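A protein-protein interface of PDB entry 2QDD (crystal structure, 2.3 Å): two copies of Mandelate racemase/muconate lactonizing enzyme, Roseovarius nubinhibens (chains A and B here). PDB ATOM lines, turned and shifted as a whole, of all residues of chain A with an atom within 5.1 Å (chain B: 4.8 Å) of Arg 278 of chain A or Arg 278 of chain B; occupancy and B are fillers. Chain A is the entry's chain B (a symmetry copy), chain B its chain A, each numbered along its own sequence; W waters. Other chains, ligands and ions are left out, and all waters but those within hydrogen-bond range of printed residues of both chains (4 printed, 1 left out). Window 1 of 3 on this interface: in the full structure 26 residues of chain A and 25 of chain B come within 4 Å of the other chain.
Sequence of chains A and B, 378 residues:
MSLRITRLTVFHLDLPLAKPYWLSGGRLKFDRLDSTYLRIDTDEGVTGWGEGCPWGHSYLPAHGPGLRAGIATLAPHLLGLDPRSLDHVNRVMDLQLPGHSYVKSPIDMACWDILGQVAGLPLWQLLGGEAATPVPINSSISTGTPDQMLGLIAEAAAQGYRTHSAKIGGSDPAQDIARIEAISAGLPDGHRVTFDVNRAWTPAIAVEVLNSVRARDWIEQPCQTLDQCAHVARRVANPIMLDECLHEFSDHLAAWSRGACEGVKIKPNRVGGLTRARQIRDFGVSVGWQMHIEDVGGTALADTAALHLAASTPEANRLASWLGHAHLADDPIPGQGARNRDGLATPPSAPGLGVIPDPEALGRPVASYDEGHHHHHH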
ATOM      1  N   TRP A 112     -25.604 -18.710  26.351  1.00  0.00           N
ATOM      2  CA  TRP A 112     -25.754 -20.143  26.072  1.00  0.00           C
ATOM      3  C   TRP A 112     -26.710 -20.812  27.071  1.00  0.00           C
ATOM      4  O   TRP A 112     -27.565 -21.613  26.678  1.00  0.00           O
ATOM      5  CB  TRP A 112     -24.391 -20.852  26.099  1.00  0.00           C
ATOM      6  CG  TRP A 112     -23.679 -20.852  24.783  1.00  0.00           C
ATOM      7  CD1 TRP A 112     -22.715 -19.979  24.378  1.00  0.00           C
ATOM      8  CD2 TRP A 112     -23.877 -21.768  23.696  1.00  0.00           C
ATOM      9  NE1 TRP A 112     -22.300 -20.287  23.104  1.00  0.00           N
ATOM     10  CE2 TRP A 112     -22.992 -21.384  22.663  1.00  0.00           C
ATOM     11  CE3 TRP A 112     -24.722 -22.870  23.491  1.00  0.00           C
ATOM     12  CZ2 TRP A 112     -22.928 -22.059  21.437  1.00  0.00           C
ATOM     13  CZ3 TRP A 112     -24.656 -23.548  22.271  1.00  0.00           C
ATOM     14  CH2 TRP A 112     -23.763 -23.138  21.259  1.00  0.00           C
ATOM     15  N   LEU A 126     -26.829 -29.040  22.274  1.00  0.00           N
ATOM     16  CA  LEU A 126     -26.736 -27.846  21.421  1.00  0.00           C
ATOM     17  C   LEU A 126     -25.376 -27.716  20.720  1.00  0.00           C
ATOM     18  O   LEU A 126     -25.283 -27.159  19.624  1.00  0.00           O
ATOM     19  CB  LEU A 126     -27.038 -26.579  22.222  1.00  0.00           C
ATOM     20  CG  LEU A 126     -28.493 -26.265  22.589  1.00  0.00           C
ATOM     21  CD1 LEU A 126     -28.528 -25.054  23.493  1.00  0.00           C
ATOM     22  CD2 LEU A 126     -29.362 -26.033  21.353  1.00  0.00           C
ATOM     23  N   LEU A 127     -24.333 -28.240  21.359  1.00  0.00           N
ATOM     24  CA  LEU A 127     -23.018 -28.372  20.746  1.00  0.00           C
ATOM     25  C   LEU A 127     -22.842 -29.687  19.962  1.00  0.00           C
ATOM     26  O   LEU A 127     -21.739 -30.020  19.528  1.00  0.00           O
ATOM     27  CB  LEU A 127     -21.920 -28.184  21.804  1.00  0.00           C
ATOM     28  CG  LEU A 127     -21.931 -26.842  22.556  1.00  0.00           C
ATOM     29  CD1 LEU A 127     -21.374 -26.966  23.958  1.00  0.00           C
ATOM     30  CD2 LEU A 127     -21.199 -25.756  21.807  1.00  0.00           C
ATOM     31  N   GLY A 128     -23.936 -30.426  19.779  1.00  0.00           N
ATOM     32  CA  GLY A 128     -24.020 -31.462  18.751  1.00  0.00           C
ATOM     33  C   GLY A 128     -23.780 -32.894  19.208  1.00  0.00           C
ATOM     34  O   GLY A 128     -23.918 -33.826  18.411  1.00  0.00           O
ATOM     35  N   LEU A 274     -17.900 -19.724  24.706  1.00  0.00           N
ATOM     36  CA  LEU A 274     -18.300 -20.978  24.086  1.00  0.00           C
ATOM     37  C   LEU A 274     -18.546 -20.897  22.585  1.00  0.00           C
ATOM     38  O   LEU A 274     -18.311 -21.869  21.880  1.00  0.00           O
ATOM     39  CB  LEU A 274     -19.533 -21.554  24.785  1.00  0.00           C
ATOM     40  CG  LEU A 274     -19.291 -22.314  26.090  1.00  0.00           C
ATOM     41  CD1 LEU A 274     -20.591 -22.460  26.848  1.00  0.00           C
ATOM     42  CD2 LEU A 274     -18.679 -23.679  25.817  1.00  0.00           C
ATOM     43  N   THR A 275     -19.034 -19.758  22.097  1.00  0.00           N
ATOM     44  CA  THR A 275     -19.286 -19.595  20.663  1.00  0.00           C
ATOM     45  C   THR A 275     -17.961 -19.622  19.891  1.00  0.00           C
ATOM     46  O   THR A 275     -17.859 -20.251  18.832  1.00  0.00           O
ATOM     47  CB  THR A 275     -20.090 -18.301  20.364  1.00  0.00           C
ATOM     48  OG1 THR A 275     -21.386 -18.392  20.973  1.00  0.00           O
ATOM     49  CG2 THR A 275     -20.268 -18.083  18.855  1.00  0.00           C
ATOM     50  N   ARG A 276     -16.946 -18.964  20.447  1.00  0.00           N
ATOM     51  CA  ARG A 276     -15.616 -18.958  19.856  1.00  0.00           C
ATOM     52  C   ARG A 276     -14.896 -20.285  20.043  1.00  0.00           C
ATOM     53  O   ARG A 276     -14.192 -20.733  19.142  1.00  0.00           O
ATOM     54  CB  ARG A 276     -14.776 -17.796  20.394  1.00  0.00           C
ATOM     55  CG  ARG A 276     -15.339 -16.396  20.084  1.00  0.00           C
ATOM     56  CD  ARG A 276     -15.154 -15.988  18.629  1.00  0.00           C
ATOM     57  NE  ARG A 276     -15.663 -14.637  18.386  1.00  0.00           N
ATOM     58  CZ  ARG A 276     -16.777 -14.357  17.712  1.00  0.00           C
ATOM     59  NH1 ARG A 276     -17.156 -13.094  17.555  1.00  0.00           N
ATOM     60  NH2 ARG A 276     -17.513 -15.334  17.188  1.00  0.00           N
ATOM     61  N   ALA A 277     -15.085 -20.917  21.197  1.00  0.00           N
ATOM     62  CA  ALA A 277     -14.476 -22.227  21.477  1.00  0.00           C
ATOM     63  C   ALA A 277     -14.983 -23.359  20.575  1.00  0.00           C
ATOM     64  O   ALA A 277     -14.211 -24.233  20.182  1.00  0.00           O
ATOM     65  CB  ALA A 277     -14.653 -22.590  22.943  1.00  0.00           C
ATOM     66  N   ARG A 278     -16.278 -23.318  20.256  1.00  0.00           N
ATOM     67  CA  ARG A 278     -16.921 -24.296  19.378  1.00  0.00           C
ATOM     68  C   ARG A 278     -16.366 -24.264  17.950  1.00  0.00           C
ATOM     69  O   ARG A 278     -16.160 -25.311  17.342  1.00  0.00           O
ATOM     70  CB  ARG A 278     -18.434 -24.056  19.350  1.00  0.00           C
ATOM     71  CG  ARG A 278     -19.231 -25.114  18.600  1.00  0.00           C
ATOM     72  CD  ARG A 278     -20.551 -24.564  18.099  1.00  0.00           C
ATOM     73  NE  ARG A 278     -21.428 -25.630  17.621  1.00  0.00           N
ATOM     74  CZ  ARG A 278     -22.749 -25.524  17.501  1.00  0.00           C
ATOM     75  NH1 ARG A 278     -23.455 -26.556  17.056  1.00  0.00           N
ATOM     76  NH2 ARG A 278     -23.370 -24.396  17.825  1.00  0.00           N
ATOM     77  N   GLN A 279     -16.152 -23.058  17.416  1.00  0.00           N
ATOM     78  CA  GLN A 279     -15.602 -22.885  16.059  1.00  0.00           C
ATOM     79  C   GLN A 279     -14.184 -23.461  15.981  1.00  0.00           C
ATOM     80  O   GLN A 279     -13.832 -24.170  15.027  1.00  0.00           O
ATOM     81  CB  GLN A 279     -15.603 -21.402  15.639  1.00  0.00           C
ATOM     82  CG  GLN A 279     -14.732 -21.118  14.392  1.00  0.00           C
ATOM     83  CD  GLN A 279     -14.712 -19.660  13.928  1.00  0.00           C
ATOM     84  OE1 GLN A 279     -14.738 -19.394  12.725  1.00  0.00           O
ATOM     85  NE2 GLN A 279     -14.633 -18.722  14.871  1.00  0.00           N
ATOM     86  N   ILE A 280     -13.388 -23.155  17.002  1.00  0.00           N
ATOM     87  CA  ILE A 280     -12.053 -23.716  17.159  1.00  0.00           C
ATOM     88  C   ILE A 280     -12.078 -25.251  17.250  1.00  0.00           C
ATOM     89  O   ILE A 280     -11.334 -25.933  16.533  1.00  0.00           O
ATOM     90  CB  ILE A 280     -11.314 -23.063  18.360  1.00  0.00           C
ATOM     91  CG1 ILE A 280     -11.049 -21.582  18.054  1.00  0.00           C
ATOM     92  CG2 ILE A 280      -9.996 -23.792  18.657  1.00  0.00           C
ATOM     93  CD1 ILE A 280     -10.807 -20.718  19.282  1.00  0.00           C
ATOM     94  N   ARG A 281     -12.954 -25.772  18.111  1.00  0.00           N
ATOM     95  CA  ARG A 281     -13.204 -27.213  18.242  1.00  0.00           C
ATOM     96  C   ARG A 281     -13.530 -27.888  16.907  1.00  0.00           C
ATOM     97  O   ARG A 281     -12.910 -28.894  16.550  1.00  0.00           O
ATOM     98  CB  ARG A 281     -14.328 -27.466  19.261  1.00  0.00           C
ATOM     99  CG  ARG A 281     -14.349 -28.869  19.867  1.00  0.00           C
ATOM    100  CD  ARG A 281     -15.200 -29.836  19.056  1.00  0.00           C
ATOM    101  NE  ARG A 281     -16.528 -29.308  18.728  1.00  0.00           N
ATOM    102  CZ  ARG A 281     -17.619 -29.519  19.461  1.00  0.00           C
ATOM    103  NH1 ARG A 281     -17.546 -30.233  20.575  1.00  0.00           N
ATOM    104  NH2 ARG A 281     -18.787 -29.015  19.086  1.00  0.00           N
ATOM    105  N   ASP A 282     -14.492 -27.324  16.179  1.00  0.00           N
ATOM    106  CA  ASP A 282     -14.890 -27.828  14.864  1.00  0.00           C
ATOM    107  C   ASP A 282     -13.752 -27.791  13.835  1.00  0.00           C
ATOM    108  O   ASP A 282     -13.601 -28.724  13.032  1.00  0.00           O
ATOM    109  CB  ASP A 282     -16.091 -27.035  14.345  1.00  0.00           C
ATOM    110  CG  ASP A 282     -17.384 -27.364  15.084  1.00  0.00           C
ATOM    111  OD1 ASP A 282     -17.376 -28.242  15.979  1.00  0.00           O
ATOM    112  OD2 ASP A 282     -18.418 -26.744  14.759  1.00  0.00           O
ATOM    113  N   PHE A 283     -12.969 -26.708  13.858  1.00  0.00           N
ATOM    114  CA  PHE A 283     -11.744 -26.603  13.054  1.00  0.00           C
ATOM    115  C   PHE A 283     -10.740 -27.703  13.399  1.00  0.00           C
ATOM    116  O   PHE A 283     -10.175 -28.327  12.503  1.00  0.00           O
ATOM    117  CB  PHE A 283     -11.078 -25.225  13.220  1.00  0.00           C
ATOM    118  CG  PHE A 283      -9.763 -25.098  12.495  1.00  0.00           C
ATOM    119  CD1 PHE A 283      -8.554 -25.247  13.175  1.00  0.00           C
ATOM    120  CD2 PHE A 283      -9.732 -24.834  11.125  1.00  0.00           C
ATOM    121  CE1 PHE A 283      -7.334 -25.131  12.501  1.00  0.00           C
ATOM    122  CE2 PHE A 283      -8.518 -24.717  10.443  1.00  0.00           C
ATOM    123  CZ  PHE A 283      -7.322 -24.865  11.132  1.00  0.00           C
ATOM    124  N   LEU A 309     -18.709 -28.757  26.209  1.00  0.00           N
ATOM    125  CA  LEU A 309     -17.959 -28.743  24.959  1.00  0.00           C
ATOM    126  C   LEU A 309     -17.088 -29.990  24.797  1.00  0.00           C
ATOM    127  O   LEU A 309     -17.060 -30.585  23.721  1.00  0.00           O
ATOM    128  CB  LEU A 309     -17.112 -27.471  24.842  1.00  0.00           C
ATOM    129  CG  LEU A 309     -16.475 -27.193  23.477  1.00  0.00           C
ATOM    130  CD1 LEU A 309     -17.511 -26.946  22.375  1.00  0.00           C
ATOM    131  CD2 LEU A 309     -15.533 -26.023  23.588  1.00  0.00           C
ATOM    132  N   ASP B  87     -24.424 -32.489  14.906  1.00  0.00           N
ATOM    133  CA  ASP B  87     -23.057 -32.881  14.588  1.00  0.00           C
ATOM    134  C   ASP B  87     -22.898 -34.396  14.619  1.00  0.00           C
ATOM    135  O   ASP B  87     -22.196 -34.960  13.782  1.00  0.00           O
ATOM    136  CB  ASP B  87     -22.058 -32.222  15.540  1.00  0.00           C
ATOM    137  CG  ASP B  87     -21.974 -30.711  15.360  1.00  0.00           C
ATOM    138  OD1 ASP B  87     -21.835 -30.233  14.212  1.00  0.00           O
ATOM    139  OD2 ASP B  87     -22.037 -29.994  16.379  1.00  0.00           O
ATOM    140  N   TRP B 112     -32.376 -30.092  10.981  1.00  0.00           N
ATOM    141  CA  TRP B 112     -32.377 -28.683  11.393  1.00  0.00           C
ATOM    142  C   TRP B 112     -33.805 -28.170  11.603  1.00  0.00           C
ATOM    143  O   TRP B 112     -34.082 -27.496  12.598  1.00  0.00           O
ATOM    144  CB  TRP B 112     -31.641 -27.799  10.367  1.00  0.00           C
ATOM    145  CG  TRP B 112     -30.154 -27.658  10.625  1.00  0.00           C
ATOM    146  CD1 TRP B 112     -29.158 -28.405  10.072  1.00  0.00           C
ATOM    147  CD2 TRP B 112     -29.508 -26.714  11.494  1.00  0.00           C
ATOM    148  NE1 TRP B 112     -27.936 -28.000  10.544  1.00  0.00           N
ATOM    149  CE2 TRP B 112     -28.116 -26.958  11.414  1.00  0.00           C
ATOM    150  CE3 TRP B 112     -29.968 -25.689  12.336  1.00  0.00           C
ATOM    151  CZ2 TRP B 112     -27.176 -26.222  12.149  1.00  0.00           C
ATOM    152  CZ3 TRP B 112     -29.031 -24.949  13.066  1.00  0.00           C
ATOM    153  CH2 TRP B 112     -27.651 -25.221  12.966  1.00  0.00           C
ATOM    154  N   LEU B 126     -31.131 -19.836  15.046  1.00  0.00           N
ATOM    155  CA  LEU B 126     -30.251 -20.940  15.445  1.00  0.00           C
ATOM    156  C   LEU B 126     -28.869 -20.804  14.815  1.00  0.00           C
ATOM    157  O   LEU B 126     -27.870 -21.225  15.399  1.00  0.00           O
ATOM    158  CB  LEU B 126     -30.864 -22.291  15.075  1.00  0.00           C
ATOM    159  CG  LEU B 126     -31.972 -22.849  15.971  1.00  0.00           C
ATOM    160  CD1 LEU B 126     -32.523 -24.116  15.351  1.00  0.00           C
ATOM    161  CD2 LEU B 126     -31.462 -23.125  17.374  1.00  0.00           C
ATOM    162  N   LEU B 127     -28.832 -20.193  13.633  1.00  0.00           N
ATOM    163  CA  LEU B 127     -27.589 -19.886  12.942  1.00  0.00           C
ATOM    164  C   LEU B 127     -26.951 -18.569  13.391  1.00  0.00           C
ATOM    165  O   LEU B 127     -25.870 -18.210  12.934  1.00  0.00           O
ATOM    166  CB  LEU B 127     -27.811 -19.917  11.424  1.00  0.00           C
ATOM    167  CG  LEU B 127     -28.166 -21.314  10.903  1.00  0.00           C
ATOM    168  CD1 LEU B 127     -28.879 -21.257   9.564  1.00  0.00           C
ATOM    169  CD2 LEU B 127     -26.942 -22.219  10.847  1.00  0.00           C
ATOM    170  N   LEU B 274     -26.509 -27.945   6.039  1.00  0.00           N
ATOM    171  CA  LEU B 274     -26.488 -26.661   6.711  1.00  0.00           C
ATOM    172  C   LEU B 274     -25.406 -26.638   7.784  1.00  0.00           C
ATOM    173  O   LEU B 274     -24.793 -25.598   8.026  1.00  0.00           O
ATOM    174  CB  LEU B 274     -27.853 -26.414   7.354  1.00  0.00           C
ATOM    175  CG  LEU B 274     -28.724 -25.201   7.029  1.00  0.00           C
ATOM    176  CD1 LEU B 274     -28.423 -24.565   5.669  1.00  0.00           C
ATOM    177  CD2 LEU B 274     -30.188 -25.624   7.118  1.00  0.00           C
ATOM    178  N   THR B 275     -25.200 -27.782   8.437  1.00  0.00           N
ATOM    179  CA  THR B 275     -24.144 -27.956   9.441  1.00  0.00           C
ATOM    180  C   THR B 275     -22.754 -27.716   8.839  1.00  0.00           C
ATOM    181  O   THR B 275     -21.950 -26.970   9.404  1.00  0.00           O
ATOM    182  CB  THR B 275     -24.216 -29.367  10.078  1.00  0.00           C
ATOM    183  OG1 THR B 275     -25.490 -29.541  10.714  1.00  0.00           O
ATOM    184  CG2 THR B 275     -23.103 -29.575  11.107  1.00  0.00           C
ATOM    185  N   ARG B 276     -22.492 -28.336   7.686  1.00  0.00           N
ATOM    186  CA  ARG B 276     -21.233 -28.148   6.971  1.00  0.00           C
ATOM    187  C   ARG B 276     -21.122 -26.737   6.382  1.00  0.00           C
ATOM    188  O   ARG B 276     -20.057 -26.127   6.436  1.00  0.00           O
ATOM    189  CB  ARG B 276     -21.058 -29.216   5.885  1.00  0.00           C
ATOM    190  CG  ARG B 276     -20.948 -30.665   6.407  1.00  0.00           C
ATOM    191  CD  ARG B 276     -19.560 -31.001   6.933  1.00  0.00           C
ATOM    192  NE  ARG B 276     -19.500 -32.334   7.534  1.00  0.00           N
ATOM    193  CZ  ARG B 276     -19.651 -32.594   8.834  1.00  0.00           C
ATOM    194  NH1 ARG B 276     -19.572 -33.844   9.273  1.00  0.00           N
ATOM    195  NH2 ARG B 276     -19.882 -31.616   9.699  1.00  0.00           N
ATOM    196  N   ALA B 277     -22.228 -26.221   5.851  1.00  0.00           N
ATOM    197  CA  ALA B 277     -22.265 -24.875   5.254  1.00  0.00           C
ATOM    198  C   ALA B 277     -22.036 -23.744   6.256  1.00  0.00           C
ATOM    199  O   ALA B 277     -21.371 -22.765   5.930  1.00  0.00           O
ATOM    200  CB  ALA B 277     -23.554 -24.660   4.493  1.00  0.00           C
ATOM    201  N   ARG B 278     -22.551 -23.905   7.475  1.00  0.00           N
ATOM    202  CA  ARG B 278     -22.340 -22.942   8.568  1.00  0.00           C
ATOM    203  C   ARG B 278     -20.876 -22.827   9.013  1.00  0.00           C
ATOM    204  O   ARG B 278     -20.383 -21.716   9.254  1.00  0.00           O
ATOM    205  CB  ARG B 278     -23.221 -23.294   9.774  1.00  0.00           C
ATOM    206  CG  ARG B 278     -23.157 -22.307  10.931  1.00  0.00           C
ATOM    207  CD  ARG B 278     -22.797 -23.018  12.222  1.00  0.00           C
ATOM    208  NE  ARG B 278     -23.794 -22.795  13.267  1.00  0.00           N
ATOM    209  CZ  ARG B 278     -24.210 -23.729  14.120  1.00  0.00           C
ATOM    210  NH1 ARG B 278     -25.122 -23.432  15.035  1.00  0.00           N
ATOM    211  NH2 ARG B 278     -23.719 -24.963  14.059  1.00  0.00           N
ATOM    212  N   GLN B 279     -20.190 -23.966   9.129  1.00  0.00           N
ATOM    213  CA  GLN B 279     -18.754 -23.979   9.433  1.00  0.00           C
ATOM    214  C   GLN B 279     -17.926 -23.218   8.393  1.00  0.00           C
ATOM    215  O   GLN B 279     -17.041 -22.440   8.750  1.00  0.00           O
ATOM    216  CB  GLN B 279     -18.214 -25.408   9.595  1.00  0.00           C
ATOM    217  CG  GLN B 279     -16.772 -25.425  10.148  1.00  0.00           C
ATOM    218  CD  GLN B 279     -16.018 -26.743   9.978  1.00  0.00           C
ATOM    219  OE1 GLN B 279     -15.044 -26.995  10.690  1.00  0.00           O
ATOM    220  NE2 GLN B 279     -16.450 -27.577   9.033  1.00  0.00           N
ATOM    221  N   ILE B 280     -18.231 -23.449   7.118  1.00  0.00           N
ATOM    222  CA  ILE B 280     -17.637 -22.709   5.998  1.00  0.00           C
ATOM    223  C   ILE B 280     -17.955 -21.206   6.034  1.00  0.00           C
ATOM    224  O   ILE B 280     -17.068 -20.369   5.823  1.00  0.00           O
ATOM    225  CB  ILE B 280     -18.060 -23.336   4.650  1.00  0.00           C
ATOM    226  CG1 ILE B 280     -17.481 -24.747   4.541  1.00  0.00           C
ATOM    227  CG2 ILE B 280     -17.613 -22.475   3.458  1.00  0.00           C
ATOM    228  CD1 ILE B 280     -18.250 -25.648   3.613  1.00  0.00           C
ATOM    229  N   ARG B 281     -19.211 -20.879   6.321  1.00  0.00           N
ATOM    230  CA  ARG B 281     -19.655 -19.491   6.469  1.00  0.00           C
ATOM    231  C   ARG B 281     -18.860 -18.757   7.542  1.00  0.00           C
ATOM    232  O   ARG B 281     -18.377 -17.646   7.313  1.00  0.00           O
ATOM    233  CB  ARG B 281     -21.152 -19.438   6.804  1.00  0.00           C
ATOM    234  CG  ARG B 281     -21.786 -18.050   6.639  1.00  0.00           C
ATOM    235  CD  ARG B 281     -21.758 -17.224   7.926  1.00  0.00           C
ATOM    236  NE  ARG B 281     -22.341 -17.910   9.089  1.00  0.00           N
ATOM    237  CZ  ARG B 281     -23.634 -17.897   9.401  1.00  0.00           C
ATOM    238  NH1 ARG B 281     -24.502 -17.258   8.627  1.00  0.00           N
ATOM    239  NH2 ARG B 281     -24.066 -18.528  10.489  1.00  0.00           N
ATOM    240  N   ASP B 282     -18.752 -19.385   8.709  1.00  0.00           N
ATOM    241  CA  ASP B 282     -18.019 -18.846   9.844  1.00  0.00           C
ATOM    242  C   ASP B 282     -16.520 -18.707   9.565  1.00  0.00           C
ATOM    243  O   ASP B 282     -15.895 -17.741  10.003  1.00  0.00           O
ATOM    244  CB  ASP B 282     -18.239 -19.735  11.074  1.00  0.00           C
ATOM    245  CG  ASP B 282     -19.649 -19.596  11.670  1.00  0.00           C
ATOM    246  OD1 ASP B 282     -20.464 -18.767  11.185  1.00  0.00           O
ATOM    247  OD2 ASP B 282     -19.937 -20.322  12.644  1.00  0.00           O
ATOM    248  N   LEU B 309     -29.375 -19.190   6.122  1.00  0.00           N
ATOM    249  CA  LEU B 309     -27.930 -19.007   6.285  1.00  0.00           C
ATOM    250  C   LEU B 309     -27.470 -17.648   5.763  1.00  0.00           C
ATOM    251  O   LEU B 309     -26.690 -16.965   6.422  1.00  0.00           O
ATOM    252  CB  LEU B 309     -27.147 -20.144   5.613  1.00  0.00           C
ATOM    253  CG  LEU B 309     -25.671 -20.296   6.015  1.00  0.00           C
ATOM    254  CD1 LEU B 309     -25.508 -20.687   7.471  1.00  0.00           C
ATOM    255  CD2 LEU B 309     -24.975 -21.305   5.127  1.00  0.00           C
HETATM  256  O   HOH W   1     -15.308 -22.195  10.946  1.00  0.00           O
HETATM  257  O   HOH W   2     -26.753 -24.617  17.366  1.00  0.00           O
HETATM  258  O   HOH W   3     -14.519 -24.332  12.301  1.00  0.00           O
HETATM  259  O   HOH W   4     -24.597 -28.857  15.936  1.00  0.00           O
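Among the printed residues, pairs that only touch across the chains: Gly 128 of chain A with Asp 87 of chain B and Phe 283 of chain A with Gln 279 of chain B.
Of the printed residues of chain B, Arg 278 of chain A touches Asp 87 (3.8 Å) and Arg 278 (3.4 Å).
Of the printed residues of chain A, Arg 278 of chain B touches Arg 278.
Printed residues of chain B within 4 Å of Phe 283 of chain A: Gln 279.
Of the printed residues of chain A, Asp 87 of chain B touches Leu 127, Gly 128 and Arg 278.
Printed residues of chain B within 4 Å of Asp 282 of chain A: Gln 279 (3.2 Å).
The nearest printed residue of chain B that does not touch Asp 282 of chain A is Asp 87 of chain B (4.9 Å).
Arg 278 of chain A touches its own counterpart, Arg 278 of chain B.
Gln 279 of chain A touches Asp 282 of chain B, and with the chains exchanged Asp 282 of chain A touches Gln 279 of chain B.
Water W4 bridges NH1 of Arg 278 of chain A (2.8 Å) and OD2 of Asp 87 of chain B (2.8 Å).
Water W1 bridges O of Gln 279 of chain B and OE1 of Gln 279 of chain A.
Water W3 lies within hydrogen-bond range of the backbone carbonyl oxygen of Gln 279 of chain A, the side-chain amide oxygen of Gln 279 of chain B and the backbone NH of Phe 283 of chain A.
Water W2 lies within hydrogen-bond range of NH1 of Arg 278 of chain B (3.1 Å) and NH2 of Arg 278 of chain A (3.4 Å).
Of the 14 printed residues of chain B, 4 touch a printed residue of chain A.
Among the printed residues, Asp or Glu carboxylates within 4 Å of a Lys or Arg side-chain nitrogen of the other chain: Arg 278 of chain A with Asp 87 of chain B.
The guanidinium group of Arg 278 of chain A lies close to the guanidinium group of Arg 278 of chain B (3.4 Å).
The side-chain amide oxygen of Gln 279 of chain B sits close to the backbone carbonyl oxygen of Asp 282 of chain A (3.2 Å).
NH1 of Arg 278 of chain A lies within salt-bridge range of OD2 of Asp 87 of chain B (3.8 Å).
The backbone carbonyl oxygen of Asp 282 of chain B lies close to the side-chain amide oxygen of Gln 279 of chain A, 3.4 Å away.
The side-chain carboxylate (OD2) of Asp 87 of chain B lies close to the backbone carbonyl oxygen (O) of Leu 127 of chain A (3.2 Å).
The backbone carbonyl oxygen of Leu 126 of chain A lies within hydrogen-bond range of the guanidinium group of Arg 278 of chain A (3.2 Å).
O of Leu 127 of chain A sits at hydrogen-bond distance from NH2 of Arg 281 of chain A, at 3.1 Å.
The guanidinium group (NE) of Arg 281 of chain A lies within salt-bridge range of the side-chain carboxylate (OD1) of Asp 282 of chain A (3.1 Å).
The guanidinium group of Arg 281 of chain B is in salt-bridge range of the side-chain carboxylate of Asp 282 of chain B (2.9 Å).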
